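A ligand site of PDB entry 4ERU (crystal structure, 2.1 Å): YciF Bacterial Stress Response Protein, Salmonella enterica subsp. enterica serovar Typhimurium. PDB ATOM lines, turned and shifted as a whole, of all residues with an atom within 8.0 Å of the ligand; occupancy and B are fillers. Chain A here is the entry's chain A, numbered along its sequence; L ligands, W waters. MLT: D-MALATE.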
ATOM      1  N   PRO A  32     -16.247 -29.594 -11.149  1.00  0.00           N
ATOM      2  CA  PRO A  32     -15.533 -28.303 -10.935  1.00  0.00           C
ATOM      3  C   PRO A  32     -16.035 -27.150 -11.817  1.00  0.00           C
ATOM      4  O   PRO A  32     -16.189 -26.016 -11.357  1.00  0.00           O
ATOM      5  CB  PRO A  32     -14.086 -28.659 -11.288  1.00  0.00           C
ATOM      6  CG  PRO A  32     -13.974 -30.117 -10.919  1.00  0.00           C
ATOM      7  CD  PRO A  32     -15.288 -30.669 -11.463  1.00  0.00           C
ATOM      8  N   LYS A  33     -16.261 -27.462 -13.089  1.00  0.00           N
ATOM      9  CA  LYS A  33     -16.799 -26.495 -14.012  1.00  0.00           C
ATOM     10  C   LYS A  33     -18.202 -26.047 -13.617  1.00  0.00           C
ATOM     11  O   LYS A  33     -18.528 -24.849 -13.704  1.00  0.00           O
ATOM     12  CB  LYS A  33     -16.829 -27.070 -15.417  1.00  0.00           C
ATOM     13  CG  LYS A  33     -17.734 -26.259 -16.303  1.00  0.00           C
ATOM     14  CD  LYS A  33     -17.078 -25.907 -17.558  1.00  0.00           C
ATOM     15  CE  LYS A  33     -17.413 -26.868 -18.618  1.00  0.00           C
ATOM     16  NZ  LYS A  33     -17.543 -26.005 -19.805  1.00  0.00           N
ATOM     17  N   LEU A  34     -19.031 -26.993 -13.166  1.00  0.00           N
ATOM     18  CA  LEU A  34     -20.370 -26.631 -12.708  1.00  0.00           C
ATOM     19  C   LEU A  34     -20.274 -25.654 -11.533  1.00  0.00           C
ATOM     20  O   LEU A  34     -21.034 -24.682 -11.476  1.00  0.00           O
ATOM     21  CB  LEU A  34     -21.205 -27.875 -12.318  1.00  0.00           C
ATOM     22  CG  LEU A  34     -21.421 -28.909 -13.424  1.00  0.00           C
ATOM     23  CD1 LEU A  34     -22.366 -30.065 -12.999  1.00  0.00           C
ATOM     24  CD2 LEU A  34     -21.919 -28.253 -14.723  1.00  0.00           C
ATOM     25  N   ALA A  35     -19.351 -25.907 -10.614  1.00  0.00           N
ATOM     26  CA  ALA A  35     -19.203 -25.022  -9.487  1.00  0.00           C
ATOM     27  C   ALA A  35     -18.800 -23.625  -9.941  1.00  0.00           C
ATOM     28  O   ALA A  35     -19.305 -22.643  -9.391  1.00  0.00           O
ATOM     29  CB  ALA A  35     -18.195 -25.579  -8.453  1.00  0.00           C
ATOM     30  N   ARG A  36     -17.946 -23.513 -10.963  1.00  0.00           N
ATOM     31  CA  ARG A  36     -17.471 -22.187 -11.437  1.00  0.00           C
ATOM     32  C   ARG A  36     -18.528 -21.437 -12.205  1.00  0.00           C
ATOM     33  O   ARG A  36     -18.600 -20.217 -12.137  1.00  0.00           O
ATOM     34  CB  ARG A  36     -16.266 -22.324 -12.376  1.00  0.00           C
ATOM     35  CG  ARG A  36     -15.056 -22.883 -11.749  1.00  0.00           C
ATOM     36  CD  ARG A  36     -13.834 -22.700 -12.656  1.00  0.00           C
ATOM     37  NE  ARG A  36     -13.909 -23.371 -13.959  1.00  0.00           N
ATOM     38  CZ  ARG A  36     -13.565 -24.636 -14.219  1.00  0.00           C
ATOM     39  NH1 ARG A  36     -13.120 -25.458 -13.274  1.00  0.00           N
ATOM     40  NH2 ARG A  36     -13.669 -25.094 -15.462  1.00  0.00           N
ATOM     41  N   ALA A  37     -19.367 -22.207 -12.924  1.00  0.00           N
ATOM     42  CA  ALA A  37     -20.337 -21.669 -13.864  1.00  0.00           C
ATOM     43  C   ALA A  37     -21.487 -20.934 -13.186  1.00  0.00           C
ATOM     44  O   ALA A  37     -22.202 -20.161 -13.816  1.00  0.00           O
ATOM     45  CB  ALA A  37     -20.866 -22.766 -14.765  1.00  0.00           C
ATOM     46  N   THR A  38     -21.667 -21.171 -11.898  1.00  0.00           N
ATOM     47  CA  THR A  38     -22.712 -20.448 -11.199  1.00  0.00           C
ATOM     48  C   THR A  38     -22.176 -19.286 -10.384  1.00  0.00           C
ATOM     49  O   THR A  38     -21.143 -19.419  -9.696  1.00  0.00           O
ATOM     50  CB  THR A  38     -23.612 -21.363 -10.328  1.00  0.00           C
ATOM     51  OG1 THR A  38     -24.446 -20.523  -9.513  1.00  0.00           O
ATOM     52  CG2 THR A  38     -22.804 -22.288  -9.444  1.00  0.00           C
ATOM     53  N   ASN A  89     -23.326 -28.940 -19.707  1.00  0.00           N
ATOM     54  CA  ASN A  89     -22.394 -28.048 -20.411  1.00  0.00           C
ATOM     55  C   ASN A  89     -23.066 -27.186 -21.458  1.00  0.00           C
ATOM     56  O   ASN A  89     -22.669 -26.032 -21.624  1.00  0.00           O
ATOM     57  CB  ASN A  89     -21.174 -28.801 -20.984  1.00  0.00           C
ATOM     58  CG  ASN A  89     -20.287 -29.365 -19.883  1.00  0.00           C
ATOM     59  OD1 ASN A  89     -20.207 -28.798 -18.787  1.00  0.00           O
ATOM     60  ND2 ASN A  89     -19.673 -30.513 -20.141  1.00  0.00           N
ATOM     61  N   VAL A  91     -26.134 -26.128 -21.228  1.00  0.00           N
ATOM     62  CA  VAL A  91     -26.770 -25.126 -20.434  1.00  0.00           C
ATOM     63  C   VAL A  91     -25.831 -23.934 -20.214  1.00  0.00           C
ATOM     64  O   VAL A  91     -26.225 -22.786 -20.395  1.00  0.00           O
ATOM     65  CB  VAL A  91     -27.298 -25.710 -19.082  1.00  0.00           C
ATOM     66  CG1 VAL A  91     -27.547 -24.597 -18.047  1.00  0.00           C
ATOM     67  CG2 VAL A  91     -28.572 -26.544 -19.354  1.00  0.00           C
ATOM     68  N   ILE A  92     -24.583 -24.214 -19.835  1.00  0.00           N
ATOM     69  CA  ILE A  92     -23.613 -23.144 -19.594  1.00  0.00           C
ATOM     70  C   ILE A  92     -23.351 -22.291 -20.842  1.00  0.00           C
ATOM     71  O   ILE A  92     -23.348 -21.054 -20.760  1.00  0.00           O
ATOM     72  CB  ILE A  92     -22.294 -23.686 -19.024  1.00  0.00           C
ATOM     73  CG1 ILE A  92     -22.553 -24.407 -17.683  1.00  0.00           C
ATOM     74  CG2 ILE A  92     -21.278 -22.562 -18.898  1.00  0.00           C
ATOM     75  CD1 ILE A  92     -21.361 -25.330 -17.255  1.00  0.00           C
ATOM     76  N   GLU A  93     -23.153 -22.928 -21.990  1.00  0.00           N
ATOM     77  CA  GLU A  93     -22.939 -22.164 -23.222  1.00  0.00           C
ATOM     78  C   GLU A  93     -24.187 -21.402 -23.686  1.00  0.00           C
ATOM     79  O   GLU A  93     -24.062 -20.415 -24.371  1.00  0.00           O
ATOM     80  CB  GLU A  93     -22.357 -23.046 -24.335  1.00  0.00           C
ATOM     81  CG  GLU A  93     -20.999 -23.658 -24.012  1.00  0.00           C
ATOM     82  CD  GLU A  93     -19.935 -22.611 -23.694  1.00  0.00           C
ATOM     83  OE1 GLU A  93     -19.789 -21.655 -24.476  1.00  0.00           O
ATOM     84  OE2 GLU A  93     -19.230 -22.750 -22.672  1.00  0.00           O
ATOM     85  N   SER A  94     -25.378 -21.842 -23.277  1.00  0.00           N
ATOM     86  CA  SER A  94     -26.625 -21.260 -23.798  1.00  0.00           C
ATOM     87  C   SER A  94     -27.273 -20.192 -22.929  1.00  0.00           C
ATOM     88  O   SER A  94     -28.415 -19.810 -23.173  1.00  0.00           O
ATOM     89  CB  SER A  94     -27.667 -22.364 -23.996  1.00  0.00           C
ATOM     90  OG  SER A  94     -27.222 -23.298 -24.956  1.00  0.00           O
ATOM     91  N   THR A  95     -26.579 -19.769 -21.880  1.00  0.00           N
ATOM     92  CA  THR A  95     -27.158 -18.845 -20.944  1.00  0.00           C
ATOM     93  C   THR A  95     -26.118 -17.839 -20.548  1.00  0.00           C
ATOM     94  O   THR A  95     -24.919 -18.042 -20.775  1.00  0.00           O
ATOM     95  CB  THR A  95     -27.647 -19.542 -19.637  1.00  0.00           C
ATOM     96  OG1 THR A  95     -26.571 -20.291 -19.053  1.00  0.00           O
ATOM     97  CG2 THR A  95     -28.865 -20.469 -19.888  1.00  0.00           C
ATOM     98  N   GLU A  96     -26.590 -16.749 -19.962  1.00  0.00           N
ATOM     99  CA  GLU A  96     -25.740 -15.817 -19.264  1.00  0.00           C
ATOM    100  C   GLU A  96     -25.538 -16.339 -17.872  1.00  0.00           C
ATOM    101  O   GLU A  96     -26.303 -17.186 -17.401  1.00  0.00           O
ATOM    102  CB  GLU A  96     -26.380 -14.423 -19.262  1.00  0.00           C
ATOM    103  CG  GLU A  96     -26.124 -13.662 -20.553  1.00  0.00           C
ATOM    104  CD  GLU A  96     -27.186 -12.643 -20.874  1.00  0.00           C
ATOM    105  OE1 GLU A  96     -28.322 -13.036 -21.218  1.00  0.00           O
ATOM    106  OE2 GLU A  96     -26.879 -11.441 -20.789  1.00  0.00           O
ATOM    107  N   LYS A  97     -24.492 -15.860 -17.203  1.00  0.00           N
ATOM    108  CA  LYS A  97     -24.223 -16.275 -15.844  1.00  0.00           C
ATOM    109  C   LYS A  97     -25.148 -15.555 -14.874  1.00  0.00           C
ATOM    110  O   LYS A  97     -24.808 -14.505 -14.338  1.00  0.00           O
ATOM    111  CB  LYS A  97     -22.741 -16.063 -15.500  1.00  0.00           C
ATOM    112  CG  LYS A  97     -22.321 -16.613 -14.140  1.00  0.00           C
ATOM    113  CD  LYS A  97     -20.796 -16.502 -13.956  1.00  0.00           C
ATOM    114  CE  LYS A  97     -20.354 -17.035 -12.588  1.00  0.00           C
ATOM    115  NZ  LYS A  97     -18.878 -16.939 -12.392  1.00  0.00           N
ATOM    116  N   ARG A 101     -29.453 -19.351 -15.551  1.00  0.00           N
ATOM    117  CA  ARG A 101     -28.488 -20.420 -15.633  1.00  0.00           C
ATOM    118  C   ARG A 101     -28.585 -21.298 -14.377  1.00  0.00           C
ATOM    119  O   ARG A 101     -28.628 -22.539 -14.467  1.00  0.00           O
ATOM    120  CB  ARG A 101     -27.054 -19.906 -15.818  1.00  0.00           C
ATOM    121  CG  ARG A 101     -26.068 -21.079 -15.992  1.00  0.00           C
ATOM    122  CD  ARG A 101     -24.628 -20.656 -15.939  1.00  0.00           C
ATOM    123  NE  ARG A 101     -24.280 -19.949 -17.158  1.00  0.00           N
ATOM    124  CZ  ARG A 101     -23.094 -19.409 -17.408  1.00  0.00           C
ATOM    125  NH1 ARG A 101     -22.106 -19.443 -16.523  1.00  0.00           N
ATOM    126  NH2 ARG A 101     -22.924 -18.812 -18.570  1.00  0.00           N
HETATM  127  C1  MLT L   1     -18.276 -20.208 -18.282  1.00  0.00           C
HETATM  128  O1  MLT L   1     -18.826 -20.174 -19.402  1.00  0.00           O
HETATM  129  O2  MLT L   1     -18.763 -19.692 -17.260  1.00  0.00           O
HETATM  130  C2  MLT L   1     -16.961 -20.931 -18.168  1.00  0.00           C
HETATM  131  O3  MLT L   1     -16.797 -21.803 -19.284  1.00  0.00           O
HETATM  132  C3  MLT L   1     -16.943 -21.745 -16.877  1.00  0.00           C
HETATM  133  C4  MLT L   1     -15.558 -22.315 -16.668  1.00  0.00           C
HETATM  134  O4  MLT L   1     -15.222 -23.324 -17.338  1.00  0.00           O
HETATM  135  O5  MLT L   1     -14.805 -21.775 -15.832  1.00  0.00           O
HETATM  136  O   HOH W   1     -15.229 -19.320 -14.419  1.00  0.00           O
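NE of Arg 36 lies within salt-bridge range of O5 of the ligand, at 2.6 Å. NH1 of Arg 101 is in salt-bridge range of O2 of the ligand, at 3.4 Å.
The side-chain amino group of Lys 97 lies within hydrogen-bond range of the backbone carbonyl oxygen of Arg 36 (3.3 Å). The guanidinium group of Arg 101 sits at hydrogen-bond distance from the backbone carbonyl oxygen of Ile 92, 3.2 Å away. The backbone carbonyl oxygen (O) of Glu 96 lies close to the guanidinium group (NE) of Arg 101 (3.4 Å). O of Ala 37 lies within hydrogen-bond range of NH1 of Arg 101 (2.8 Å). OG1 of Thr 95 sits at hydrogen-bond distance from NE of Arg 101 (3.0 Å).
Residues that only touch the ligand: Lys 33 and Ile 92. Four residues have an atom within 4 Å of the ligand: Lys 33, Arg 36, Ile 92 and Arg 101. The nearest printed residue that does not touch the ligand is Glu 93 (4.2 Å).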
